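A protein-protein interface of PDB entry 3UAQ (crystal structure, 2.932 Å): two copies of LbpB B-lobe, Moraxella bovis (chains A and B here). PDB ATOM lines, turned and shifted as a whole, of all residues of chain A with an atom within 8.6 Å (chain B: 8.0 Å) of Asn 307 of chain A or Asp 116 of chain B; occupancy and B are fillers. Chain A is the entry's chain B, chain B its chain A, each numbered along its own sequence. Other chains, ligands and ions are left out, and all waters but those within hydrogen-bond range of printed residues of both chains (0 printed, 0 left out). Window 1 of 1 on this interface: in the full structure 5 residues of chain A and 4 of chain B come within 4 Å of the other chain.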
ATOM      1  N   ASP A 274     -35.688 -32.174 -22.551  1.00  0.00           N
ATOM      2  CA  ASP A 274     -35.492 -32.080 -23.992  1.00  0.00           C
ATOM      3  C   ASP A 274     -34.228 -32.825 -24.392  1.00  0.00           C
ATOM      4  O   ASP A 274     -33.137 -32.258 -24.379  1.00  0.00           O
ATOM      5  CB  ASP A 274     -35.387 -30.613 -24.408  1.00  0.00           C
ATOM      6  CG  ASP A 274     -35.274 -30.439 -25.906  1.00  0.00           C
ATOM      7  OD1 ASP A 274     -35.853 -31.265 -26.644  1.00  0.00           O
ATOM      8  OD2 ASP A 274     -34.613 -29.473 -26.344  1.00  0.00           O
ATOM      9  N   ALA A 275     -34.382 -34.095 -24.753  1.00  0.00           N
ATOM     10  CA  ALA A 275     -33.232 -34.942 -25.041  1.00  0.00           C
ATOM     11  C   ALA A 275     -33.326 -35.638 -26.394  1.00  0.00           C
ATOM     12  O   ALA A 275     -34.416 -35.947 -26.877  1.00  0.00           O
ATOM     13  CB  ALA A 275     -33.025 -35.962 -23.930  1.00  0.00           C
ATOM     14  N   THR A 276     -32.168 -35.879 -26.996  1.00  0.00           N
ATOM     15  CA  THR A 276     -32.093 -36.665 -28.217  1.00  0.00           C
ATOM     16  C   THR A 276     -31.779 -38.119 -27.887  1.00  0.00           C
ATOM     17  O   THR A 276     -30.980 -38.399 -26.989  1.00  0.00           O
ATOM     18  CB  THR A 276     -31.029 -36.120 -29.178  1.00  0.00           C
ATOM     19  OG1 THR A 276     -31.476 -34.870 -29.722  1.00  0.00           O
ATOM     20  CG2 THR A 276     -30.773 -37.117 -30.311  1.00  0.00           C
ATOM     21  N   ALA A 283     -29.624 -38.101 -24.401  1.00  0.00           N
ATOM     22  CA  ALA A 283     -28.912 -36.993 -23.769  1.00  0.00           C
ATOM     23  C   ALA A 283     -29.404 -35.648 -24.282  1.00  0.00           C
ATOM     24  O   ALA A 283     -29.743 -35.500 -25.458  1.00  0.00           O
ATOM     25  CB  ALA A 283     -27.418 -37.123 -23.991  1.00  0.00           C
ATOM     26  N   GLY A 284     -29.445 -34.668 -23.390  1.00  0.00           N
ATOM     27  CA  GLY A 284     -29.902 -33.347 -23.754  1.00  0.00           C
ATOM     28  C   GLY A 284     -29.948 -32.393 -22.583  1.00  0.00           C
ATOM     29  O   GLY A 284     -28.997 -32.283 -21.801  1.00  0.00           O
ATOM     30  N   SER A 285     -31.072 -31.702 -22.459  1.00  0.00           N
ATOM     31  CA  SER A 285     -31.172 -30.603 -21.517  1.00  0.00           C
ATOM     32  C   SER A 285     -32.363 -30.724 -20.572  1.00  0.00           C
ATOM     33  O   SER A 285     -33.418 -31.270 -20.935  1.00  0.00           O
ATOM     34  CB  SER A 285     -31.247 -29.274 -22.274  1.00  0.00           C
ATOM     35  OG  SER A 285     -30.181 -29.153 -23.196  1.00  0.00           O
ATOM     36  N   ALA A 286     -32.168 -30.214 -19.357  1.00  0.00           N
ATOM     37  CA  ALA A 286     -33.255 -29.962 -18.419  1.00  0.00           C
ATOM     38  C   ALA A 286     -33.507 -28.457 -18.402  1.00  0.00           C
ATOM     39  O   ALA A 286     -32.569 -27.665 -18.263  1.00  0.00           O
ATOM     40  CB  ALA A 286     -32.884 -30.451 -17.031  1.00  0.00           C
ATOM     41  N   ILE A 287     -34.769 -28.061 -18.550  1.00  0.00           N
ATOM     42  CA  ILE A 287     -35.116 -26.649 -18.663  1.00  0.00           C
ATOM     43  C   ILE A 287     -35.942 -26.198 -17.465  1.00  0.00           C
ATOM     44  O   ILE A 287     -36.987 -26.777 -17.164  1.00  0.00           O
ATOM     45  CB  ILE A 287     -35.891 -26.358 -19.973  1.00  0.00           C
ATOM     46  CG1 ILE A 287     -34.986 -26.569 -21.191  1.00  0.00           C
ATOM     47  CG2 ILE A 287     -36.444 -24.945 -19.970  1.00  0.00           C
ATOM     48  CD1 ILE A 287     -35.317 -27.807 -22.001  1.00  0.00           C
ATOM     49  N   ASN A 304     -31.113 -24.019 -15.804  1.00  0.00           N
ATOM     50  CA  ASN A 304     -31.173 -25.203 -16.643  1.00  0.00           C
ATOM     51  C   ASN A 304     -30.003 -26.128 -16.375  1.00  0.00           C
ATOM     52  O   ASN A 304     -29.084 -25.795 -15.620  1.00  0.00           O
ATOM     53  CB  ASN A 304     -31.122 -24.818 -18.123  1.00  0.00           C
ATOM     54  CG  ASN A 304     -32.293 -23.962 -18.552  1.00  0.00           C
ATOM     55  OD1 ASN A 304     -33.181 -23.655 -17.757  1.00  0.00           O
ATOM     56  ND2 ASN A 304     -32.298 -23.568 -19.821  1.00  0.00           N
ATOM     57  N   ALA A 305     -30.059 -27.299 -16.998  1.00  0.00           N
ATOM     58  CA  ALA A 305     -28.885 -28.120 -17.215  1.00  0.00           C
ATOM     59  C   ALA A 305     -28.796 -28.280 -18.730  1.00  0.00           C
ATOM     60  O   ALA A 305     -29.219 -29.294 -19.288  1.00  0.00           O
ATOM     61  CB  ALA A 305     -29.025 -29.471 -16.530  1.00  0.00           C
ATOM     62  N   ASP A 306     -28.276 -27.251 -19.396  1.00  0.00           N
ATOM     63  CA  ASP A 306     -28.192 -27.243 -20.851  1.00  0.00           C
ATOM     64  C   ASP A 306     -27.140 -28.241 -21.314  1.00  0.00           C
ATOM     65  O   ASP A 306     -25.956 -28.106 -20.993  1.00  0.00           O
ATOM     66  CB  ASP A 306     -27.861 -25.840 -21.369  1.00  0.00           C
ATOM     67  CG  ASP A 306     -28.907 -24.809 -20.976  1.00  0.00           C
ATOM     68  OD1 ASP A 306     -30.060 -24.915 -21.449  1.00  0.00           O
ATOM     69  OD2 ASP A 306     -28.569 -23.881 -20.210  1.00  0.00           O
ATOM     70  N   ASN A 307     -27.579 -29.250 -22.058  1.00  0.00           N
ATOM     71  CA  ASN A 307     -26.675 -30.296 -22.503  1.00  0.00           C
ATOM     72  C   ASN A 307     -25.948 -30.926 -21.330  1.00  0.00           C
ATOM     73  O   ASN A 307     -24.765 -31.249 -21.431  1.00  0.00           O
ATOM     74  CB  ASN A 307     -25.652 -29.731 -23.491  1.00  0.00           C
ATOM     75  CG  ASN A 307     -26.198 -29.627 -24.893  1.00  0.00           C
ATOM     76  OD1 ASN A 307     -26.723 -30.598 -25.440  1.00  0.00           O
ATOM     77  ND2 ASN A 307     -26.091 -28.443 -25.480  1.00  0.00           N
ATOM     78  N   ARG A 308     -26.654 -31.075 -20.212  1.00  0.00           N
ATOM     79  CA  ARG A 308     -26.080 -31.670 -19.011  1.00  0.00           C
ATOM     80  C   ARG A 308     -27.037 -32.689 -18.403  1.00  0.00           C
ATOM     81  O   ARG A 308     -27.000 -32.955 -17.199  1.00  0.00           O
ATOM     82  CB  ARG A 308     -25.723 -30.586 -17.991  1.00  0.00           C
ATOM     83  CG  ARG A 308     -24.598 -29.670 -18.455  1.00  0.00           C
ATOM     84  CD  ARG A 308     -24.563 -28.370 -17.670  1.00  0.00           C
ATOM     85  NE  ARG A 308     -24.181 -28.565 -16.276  1.00  0.00           N
ATOM     86  CZ  ARG A 308     -22.921 -28.605 -15.851  1.00  0.00           C
ATOM     87  NH1 ARG A 308     -21.924 -28.475 -16.719  1.00  0.00           N
ATOM     88  NH2 ARG A 308     -22.653 -28.777 -14.561  1.00  0.00           N
ATOM     89  N   LEU A 309     -27.896 -33.255 -19.246  1.00  0.00           N
ATOM     90  CA  LEU A 309     -28.779 -34.338 -18.833  1.00  0.00           C
ATOM     91  C   LEU A 309     -28.468 -35.586 -19.655  1.00  0.00           C
ATOM     92  O   LEU A 309     -28.331 -35.509 -20.877  1.00  0.00           O
ATOM     93  CB  LEU A 309     -30.240 -33.936 -19.025  1.00  0.00           C
ATOM     94  CG  LEU A 309     -31.273 -35.042 -18.789  1.00  0.00           C
ATOM     95  CD1 LEU A 309     -32.492 -34.498 -18.058  1.00  0.00           C
ATOM     96  CD2 LEU A 309     -31.672 -35.723 -20.098  1.00  0.00           C
ATOM     97  N   GLU A 310     -28.350 -36.732 -18.987  1.00  0.00           N
ATOM     98  CA  GLU A 310     -28.075 -37.991 -19.674  1.00  0.00           C
ATOM     99  C   GLU A 310     -28.913 -39.109 -19.076  1.00  0.00           C
ATOM    100  O   GLU A 310     -29.385 -38.999 -17.946  1.00  0.00           O
ATOM    101  CB  GLU A 310     -26.580 -38.331 -19.595  1.00  0.00           C
ATOM    102  CG  GLU A 310     -26.149 -39.019 -18.312  1.00  0.00           C
ATOM    103  CD  GLU A 310     -26.240 -40.520 -18.416  1.00  0.00           C
ATOM    104  OE1 GLU A 310     -26.084 -41.041 -19.545  1.00  0.00           O
ATOM    105  OE2 GLU A 310     -26.470 -41.176 -17.375  1.00  0.00           O
ATOM    106  N   LYS A 324     -29.929 -38.784 -15.116  1.00  0.00           N
ATOM    107  CA  LYS A 324     -29.524 -37.733 -14.198  1.00  0.00           C
ATOM    108  C   LYS A 324     -29.251 -36.461 -14.973  1.00  0.00           C
ATOM    109  O   LYS A 324     -29.086 -36.483 -16.190  1.00  0.00           O
ATOM    110  CB  LYS A 324     -28.233 -38.134 -13.485  1.00  0.00           C
ATOM    111  CG  LYS A 324     -27.105 -38.508 -14.445  1.00  0.00           C
ATOM    112  CD  LYS A 324     -25.769 -37.913 -14.008  1.00  0.00           C
ATOM    113  CE  LYS A 324     -24.694 -38.158 -15.068  1.00  0.00           C
ATOM    114  NZ  LYS A 324     -24.564 -39.590 -15.447  1.00  0.00           N
ATOM    115  N   PHE A 325     -29.200 -35.348 -14.260  1.00  0.00           N
ATOM    116  CA  PHE A 325     -28.683 -34.112 -14.820  1.00  0.00           C
ATOM    117  C   PHE A 325     -28.119 -33.253 -13.695  1.00  0.00           C
ATOM    118  O   PHE A 325     -28.505 -33.399 -12.528  1.00  0.00           O
ATOM    119  CB  PHE A 325     -29.755 -33.361 -15.618  1.00  0.00           C
ATOM    120  CG  PHE A 325     -30.856 -32.771 -14.773  1.00  0.00           C
ATOM    121  CD1 PHE A 325     -30.633 -31.645 -13.991  1.00  0.00           C
ATOM    122  CD2 PHE A 325     -32.123 -33.324 -14.787  1.00  0.00           C
ATOM    123  CE1 PHE A 325     -31.653 -31.105 -13.222  1.00  0.00           C
ATOM    124  CE2 PHE A 325     -33.142 -32.785 -14.025  1.00  0.00           C
ATOM    125  CZ  PHE A 325     -32.907 -31.677 -13.244  1.00  0.00           C
ATOM    126  N   LEU A 326     -27.177 -32.388 -14.048  1.00  0.00           N
ATOM    127  CA  LEU A 326     -26.592 -31.460 -13.098  1.00  0.00           C
ATOM    128  C   LEU A 326     -26.587 -30.077 -13.722  1.00  0.00           C
ATOM    129  O   LEU A 326     -26.098 -29.889 -14.842  1.00  0.00           O
ATOM    130  CB  LEU A 326     -25.171 -31.875 -12.740  1.00  0.00           C
ATOM    131  CG  LEU A 326     -24.415 -30.864 -11.868  1.00  0.00           C
ATOM    132  CD1 LEU A 326     -24.935 -30.863 -10.430  1.00  0.00           C
ATOM    133  CD2 LEU A 326     -22.917 -31.134 -11.899  1.00  0.00           C
ATOM    134  N   THR A 327     -27.139 -29.113 -12.997  1.00  0.00           N
ATOM    135  CA  THR A 327     -27.381 -27.791 -13.552  1.00  0.00           C
ATOM    136  C   THR A 327     -26.109 -27.040 -13.971  1.00  0.00           C
ATOM    137  O   THR A 327     -24.986 -27.441 -13.642  1.00  0.00           O
ATOM    138  CB  THR A 327     -28.206 -26.941 -12.588  1.00  0.00           C
ATOM    139  OG1 THR A 327     -27.640 -27.022 -11.274  1.00  0.00           O
ATOM    140  CG2 THR A 327     -29.632 -27.456 -12.546  1.00  0.00           C
ATOM    141  N   ASN A 328     -26.312 -25.944 -14.700  1.00  0.00           N
ATOM    142  CA  ASN A 328     -25.221 -25.148 -15.255  1.00  0.00           C
ATOM    143  C   ASN A 328     -24.280 -24.580 -14.200  1.00  0.00           C
ATOM    144  O   ASN A 328     -23.062 -24.582 -14.386  1.00  0.00           O
ATOM    145  CB  ASN A 328     -25.767 -24.010 -16.127  1.00  0.00           C
ATOM    146  CG  ASN A 328     -26.369 -24.505 -17.428  1.00  0.00           C
ATOM    147  OD1 ASN A 328     -26.198 -25.666 -17.807  1.00  0.00           O
ATOM    148  ND2 ASN A 328     -27.074 -23.621 -18.124  1.00  0.00           N
ATOM    149  N   ASN B  93     -13.129 -28.292 -28.209  1.00  0.00           N
ATOM    150  CA  ASN B  93     -13.847 -27.331 -27.377  1.00  0.00           C
ATOM    151  C   ASN B  93     -12.877 -26.447 -26.582  1.00  0.00           C
ATOM    152  O   ASN B  93     -12.212 -26.915 -25.658  1.00  0.00           O
ATOM    153  CB  ASN B  93     -14.811 -28.064 -26.441  1.00  0.00           C
ATOM    154  CG  ASN B  93     -15.670 -27.119 -25.635  1.00  0.00           C
ATOM    155  OD1 ASN B  93     -15.835 -25.951 -25.995  1.00  0.00           O
ATOM    156  ND2 ASN B  93     -16.227 -27.618 -24.537  1.00  0.00           N
ATOM    157  N   LEU B  95     -13.372 -23.898 -24.579  1.00  0.00           N
ATOM    158  CA  LEU B  95     -13.834 -23.302 -23.321  1.00  0.00           C
ATOM    159  C   LEU B  95     -13.123 -23.800 -22.057  1.00  0.00           C
ATOM    160  O   LEU B  95     -12.792 -23.000 -21.193  1.00  0.00           O
ATOM    161  CB  LEU B  95     -15.353 -23.404 -23.188  1.00  0.00           C
ATOM    162  CG  LEU B  95     -16.017 -22.243 -23.929  1.00  0.00           C
ATOM    163  CD1 LEU B  95     -17.013 -22.721 -24.976  1.00  0.00           C
ATOM    164  CD2 LEU B  95     -16.661 -21.285 -22.948  1.00  0.00           C
ATOM    165  N   GLN B 113     -19.969 -16.175 -19.015  1.00  0.00           N
ATOM    166  CA  GLN B 113     -19.888 -16.814 -20.318  1.00  0.00           C
ATOM    167  C   GLN B 113     -21.272 -17.018 -20.913  1.00  0.00           C
ATOM    168  O   GLN B 113     -22.279 -16.995 -20.198  1.00  0.00           O
ATOM    169  CB  GLN B 113     -19.172 -18.158 -20.193  1.00  0.00           C
ATOM    170  CG  GLN B 113     -19.669 -19.010 -19.027  1.00  0.00           C
ATOM    171  CD  GLN B 113     -18.943 -20.336 -18.919  1.00  0.00           C
ATOM    172  OE1 GLN B 113     -18.924 -21.128 -19.867  1.00  0.00           O
ATOM    173  NE2 GLN B 113     -18.338 -20.589 -17.759  1.00  0.00           N
ATOM    174  N   SER B 114     -21.309 -17.222 -22.227  1.00  0.00           N
ATOM    175  CA  SER B 114     -22.564 -17.385 -22.946  1.00  0.00           C
ATOM    176  C   SER B 114     -23.262 -18.682 -22.559  1.00  0.00           C
ATOM    177  O   SER B 114     -22.610 -19.654 -22.181  1.00  0.00           O
ATOM    178  CB  SER B 114     -22.313 -17.339 -24.454  1.00  0.00           C
ATOM    179  OG  SER B 114     -22.085 -16.009 -24.894  1.00  0.00           O
ATOM    180  N   ASP B 115     -24.590 -18.685 -22.647  1.00  0.00           N
ATOM    181  CA  ASP B 115     -25.383 -19.879 -22.350  1.00  0.00           C
ATOM    182  C   ASP B 115     -25.234 -20.931 -23.446  1.00  0.00           C
ATOM    183  O   ASP B 115     -25.274 -20.609 -24.634  1.00  0.00           O
ATOM    184  CB  ASP B 115     -26.856 -19.510 -22.155  1.00  0.00           C
ATOM    185  CG  ASP B 115     -27.131 -18.917 -20.785  1.00  0.00           C
ATOM    186  OD1 ASP B 115     -26.168 -18.470 -20.123  1.00  0.00           O
ATOM    187  OD2 ASP B 115     -28.311 -18.900 -20.371  1.00  0.00           O
ATOM    188  N   ASP B 116     -25.056 -22.185 -23.043  1.00  0.00           N
ATOM    189  CA  ASP B 116     -24.832 -23.266 -23.998  1.00  0.00           C
ATOM    190  C   ASP B 116     -26.157 -23.873 -24.444  1.00  0.00           C
ATOM    191  O   ASP B 116     -26.595 -24.890 -23.906  1.00  0.00           O
ATOM    192  CB  ASP B 116     -23.921 -24.340 -23.391  1.00  0.00           C
ATOM    193  CG  ASP B 116     -23.340 -25.269 -24.439  1.00  0.00           C
ATOM    194  OD1 ASP B 116     -23.521 -24.991 -25.645  1.00  0.00           O
ATOM    195  OD2 ASP B 116     -22.698 -26.272 -24.059  1.00  0.00           O
ATOM    196  N   LYS B 117     -26.795 -23.251 -25.430  1.00  0.00           N
ATOM    197  CA  LYS B 117     -28.148 -23.653 -25.812  1.00  0.00           C
ATOM    198  C   LYS B 117     -28.295 -24.246 -27.222  1.00  0.00           C
ATOM    199  O   LYS B 117     -29.408 -24.319 -27.755  1.00  0.00           O
ATOM    200  CB  LYS B 117     -29.134 -22.505 -25.588  1.00  0.00           C
ATOM    201  CG  LYS B 117     -29.783 -22.569 -24.209  1.00  0.00           C
ATOM    202  CD  LYS B 117     -30.272 -21.216 -23.729  1.00  0.00           C
ATOM    203  CE  LYS B 117     -30.972 -21.352 -22.373  1.00  0.00           C
ATOM    204  NZ  LYS B 117     -31.333 -20.040 -21.763  1.00  0.00           N
ATOM    205  N   TYR B 118     -27.181 -24.683 -27.805  1.00  0.00           N
ATOM    206  CA  TYR B 118     -27.204 -25.465 -29.041  1.00  0.00           C
ATOM    207  C   TYR B 118     -26.699 -26.876 -28.764  1.00  0.00           C
ATOM    208  O   TYR B 118     -26.153 -27.139 -27.695  1.00  0.00           O
ATOM    209  CB  TYR B 118     -26.360 -24.792 -30.124  1.00  0.00           C
ATOM    210  CG  TYR B 118     -26.839 -23.407 -30.475  1.00  0.00           C
ATOM    211  CD1 TYR B 118     -27.599 -23.176 -31.615  1.00  0.00           C
ATOM    212  CD2 TYR B 118     -26.544 -22.330 -29.658  1.00  0.00           C
ATOM    213  CE1 TYR B 118     -28.046 -21.901 -31.931  1.00  0.00           C
ATOM    214  CE2 TYR B 118     -26.985 -21.052 -29.964  1.00  0.00           C
ATOM    215  CZ  TYR B 118     -27.733 -20.844 -31.099  1.00  0.00           C
ATOM    216  OH  TYR B 118     -28.166 -19.574 -31.399  1.00  0.00           O
ATOM    217  N   LYS B 119     -26.861 -27.776 -29.729  1.00  0.00           N
ATOM    218  CA  LYS B 119     -26.575 -29.188 -29.494  1.00  0.00           C
ATOM    219  C   LYS B 119     -25.175 -29.617 -29.924  1.00  0.00           C
ATOM    220  O   LYS B 119     -24.515 -30.407 -29.243  1.00  0.00           O
ATOM    221  CB  LYS B 119     -27.620 -30.069 -30.179  1.00  0.00           C
ATOM    222  CG  LYS B 119     -27.244 -31.542 -30.190  1.00  0.00           C
ATOM    223  CD  LYS B 119     -28.463 -32.439 -30.127  1.00  0.00           C
ATOM    224  CE  LYS B 119     -28.158 -33.740 -29.396  1.00  0.00           C
ATOM    225  NZ  LYS B 119     -28.564 -33.683 -27.963  1.00  0.00           N
ATOM    226  N   PHE B 120     -24.736 -29.107 -31.068  1.00  0.00           N
ATOM    227  CA  PHE B 120     -23.435 -29.459 -31.619  1.00  0.00           C
ATOM    228  C   PHE B 120     -22.551 -28.228 -31.592  1.00  0.00           C
ATOM    229  O   PHE B 120     -21.325 -28.320 -31.658  1.00  0.00           O
ATOM    230  CB  PHE B 120     -23.578 -29.922 -33.073  1.00  0.00           C
ATOM    231  CG  PHE B 120     -24.457 -31.132 -33.253  1.00  0.00           C
ATOM    232  CD1 PHE B 120     -23.913 -32.407 -33.229  1.00  0.00           C
ATOM    233  CD2 PHE B 120     -25.822 -30.994 -33.457  1.00  0.00           C
ATOM    234  CE1 PHE B 120     -24.713 -33.520 -33.397  1.00  0.00           C
ATOM    235  CE2 PHE B 120     -26.629 -32.102 -33.625  1.00  0.00           C
ATOM    236  CZ  PHE B 120     -26.075 -33.369 -33.596  1.00  0.00           C
ATOM    237  N   VAL B 121     -23.191 -27.070 -31.473  1.00  0.00           N
ATOM    238  CA  VAL B 121     -22.547 -25.800 -31.785  1.00  0.00           C
ATOM    239  C   VAL B 121     -22.391 -24.876 -30.576  1.00  0.00           C
ATOM    240  O   VAL B 121     -23.228 -24.854 -29.667  1.00  0.00           O
ATOM    241  CB  VAL B 121     -23.321 -25.077 -32.903  1.00  0.00           C
ATOM    242  CG1 VAL B 121     -23.454 -23.592 -32.613  1.00  0.00           C
ATOM    243  CG2 VAL B 121     -22.662 -25.314 -34.246  1.00  0.00           C
ATOM    244  N   LYS B 122     -21.303 -24.113 -30.584  1.00  0.00           N
ATOM    245  CA  LYS B 122     -21.080 -23.071 -29.598  1.00  0.00           C
ATOM    246  C   LYS B 122     -20.686 -21.777 -30.298  1.00  0.00           C
ATOM    247  O   LYS B 122     -19.995 -21.794 -31.311  1.00  0.00           O
ATOM    248  CB  LYS B 122     -19.978 -23.490 -28.629  1.00  0.00           C
ATOM    249  CG  LYS B 122     -19.974 -24.973 -28.306  1.00  0.00           C
ATOM    250  CD  LYS B 122     -19.405 -25.240 -26.925  1.00  0.00           C
ATOM    251  CE  LYS B 122     -19.744 -26.644 -26.472  1.00  0.00           C
ATOM    252  NZ  LYS B 122     -20.055 -26.687 -25.020  1.00  0.00           N
ATOM    253  N   ALA B 123     -21.140 -20.654 -29.760  1.00  0.00           N
ATOM    254  CA  ALA B 123     -20.685 -19.351 -30.223  1.00  0.00           C
ATOM    255  C   ALA B 123     -21.038 -18.337 -29.161  1.00  0.00           C
ATOM    256  O   ALA B 123     -22.169 -18.314 -28.667  1.00  0.00           O
ATOM    257  CB  ALA B 123     -21.347 -18.978 -31.537  1.00  0.00           C
ATOM    258  N   TYR B 156     -15.676 -16.631 -29.137  1.00  0.00           N
ATOM    259  CA  TYR B 156     -15.421 -17.934 -29.736  1.00  0.00           C
ATOM    260  C   TYR B 156     -16.567 -18.437 -30.611  1.00  0.00           C
ATOM    261  O   TYR B 156     -17.712 -17.971 -30.512  1.00  0.00           O
ATOM    262  CB  TYR B 156     -15.146 -18.958 -28.633  1.00  0.00           C
ATOM    263  CG  TYR B 156     -16.328 -19.120 -27.705  1.00  0.00           C
ATOM    264  CD1 TYR B 156     -17.353 -20.000 -28.010  1.00  0.00           C
ATOM    265  CD2 TYR B 156     -16.432 -18.377 -26.533  1.00  0.00           C
ATOM    266  CE1 TYR B 156     -18.445 -20.149 -27.171  1.00  0.00           C
ATOM    267  CE2 TYR B 156     -17.524 -18.520 -25.686  1.00  0.00           C
ATOM    268  CZ  TYR B 156     -18.529 -19.409 -26.012  1.00  0.00           C
ATOM    269  OH  TYR B 156     -19.622 -19.562 -25.180  1.00  0.00           O
ATOM    270  N   HIS B 176     -28.426 -16.898 -32.911  1.00  0.00           N
ATOM    271  CA  HIS B 176     -27.896 -15.641 -32.411  1.00  0.00           C
ATOM    272  C   HIS B 176     -26.511 -15.333 -32.963  1.00  0.00           C
ATOM    273  O   HIS B 176     -25.931 -16.132 -33.705  1.00  0.00           O
ATOM    274  CB  HIS B 176     -27.811 -15.696 -30.890  1.00  0.00           C
ATOM    275  CG  HIS B 176     -26.613 -16.434 -30.389  1.00  0.00           C
ATOM    276  ND1 HIS B 176     -26.425 -17.787 -30.603  1.00  0.00           N
ATOM    277  CD2 HIS B 176     -25.525 -16.010 -29.701  1.00  0.00           C
ATOM    278  CE1 HIS B 176     -25.284 -18.160 -30.059  1.00  0.00           C
ATOM    279  NE2 HIS B 176     -24.716 -17.104 -29.504  1.00  0.00           N
ATOM    280  N   GLN B 233     -27.748 -11.084 -22.519  1.00  0.00           N
ATOM    281  CA  GLN B 233     -27.879 -12.136 -23.523  1.00  0.00           C
ATOM    282  C   GLN B 233     -29.238 -12.113 -24.208  1.00  0.00           C
ATOM    283  O   GLN B 233     -30.224 -11.648 -23.633  1.00  0.00           O
ATOM    284  CB  GLN B 233     -27.646 -13.518 -22.896  1.00  0.00           C
ATOM    285  CG  GLN B 233     -26.199 -13.822 -22.542  1.00  0.00           C
ATOM    286  CD  GLN B 233     -25.999 -15.276 -22.148  1.00  0.00           C
ATOM    287  OE1 GLN B 233     -26.309 -16.188 -22.917  1.00  0.00           O
ATOM    288  NE2 GLN B 233     -25.482 -15.500 -20.943  1.00  0.00           N
ATOM    289  N   GLU B 320     -27.414 -27.896 -37.370  1.00  0.00           N
ATOM    290  CA  GLU B 320     -26.985 -26.594 -36.862  1.00  0.00           C
ATOM    291  C   GLU B 320     -25.914 -25.961 -37.750  1.00  0.00           C
ATOM    292  O   GLU B 320     -25.374 -26.605 -38.657  1.00  0.00           O
ATOM    293  CB  GLU B 320     -26.494 -26.702 -35.408  1.00  0.00           C
ATOM    294  CG  GLU B 320     -27.586 -27.061 -34.395  1.00  0.00           C
ATOM    295  CD  GLU B 320     -27.057 -27.231 -32.981  1.00  0.00           C
ATOM    296  OE1 GLU B 320     -25.824 -27.179 -32.784  1.00  0.00           O
ATOM    297  OE2 GLU B 320     -27.878 -27.418 -32.060  1.00  0.00           O
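Of the 17 printed residues of chain B, 4 touch a printed residue of chain A.
Printed residues of chain B that touch a printed residue of chain A: Asp 116, Lys 117, Tyr 118 and Lys 119.
Among the printed residues, 7 pairs touch across the chains.
Among the printed residues, no Asp or Glu carboxylate lies within 4 Å of a Lys or Arg side-chain nitrogen of the other chain.
No position is printed for both chains.
Of chain B, only Asp 116 and Tyr 118 come within 4 Å of Asn 307 of chain A.
Of chain A, only Asp 306 (3.0 Å) and Asn 307 (3.9 Å) come within 4 Å of Asp 116 of chain B.
Of the printed residues of chain A, Tyr 118 of chain B touches Asn 307.
Printed residues of chain A within 4 Å of Lys 119 of chain B: Thr 276 and Ala 283.
Of the printed residues of chain B, Ala 283 of chain A touches Lys 119 (3.3 Å).
Printed residues of chain B within 4 Å of Asn 304 of chain A: Lys 117.
The nearest residue of chain A that does not touch Asp 116 of chain B is Asn 328 of chain A (5.5 Å).
The side-chain amide nitrogen (ND2) of Asn 307 of chain A lies within hydrogen-bond range of the backbone carbonyl oxygen (O) of Tyr 118 of chain B, 2.6 Å away.
The side-chain amino group (NZ) of Lys 119 of chain B lies within hydrogen-bond range of the backbone carbonyl oxygen (O) of Ala 283 of chain A.
CE of Lys 119 of chain B touches OG1 of Thr 276 of chain A, 3.5 Å away.
Asn 304 of chain A touches Lys 117 of chain B.
Asp 116 of chain B touches Asp 306 of chain A (O to CB, 3.0 Å).
Lys 117 of chain B touches Asp 306 of chain A.
ND2 of Asn 307 of chain A touches O of Asp 116 of chain B, 3.9 Å away.
OD2 of Asp 116 of chain B is in salt-bridge range of NZ of Lys 122 of chain B (2.8 Å).
ND1 of His 176 of chain B sits at hydrogen-bond distance from OH of Tyr 118 of chain B (2.6 Å).
The backbone NH of Lys 119 of chain B lies within hydrogen-bond range of the side-chain carboxylate of Glu 320 of chain B.
The backbone carbonyl oxygen of Gly 284 of chain A sits close to the backbone NH of Asn 307 of chain A (3.4 Å).
O of Asn 304 of chain A sits at hydrogen-bond distance from N of Asn 328 of chain A, 2.9 Å away.
The side-chain amide nitrogen (ND2) of Asn 328 of chain A is in hydrogen-bond range of the side-chain carboxylate (OD2) of Asp 306 of chain A (2.6 Å).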
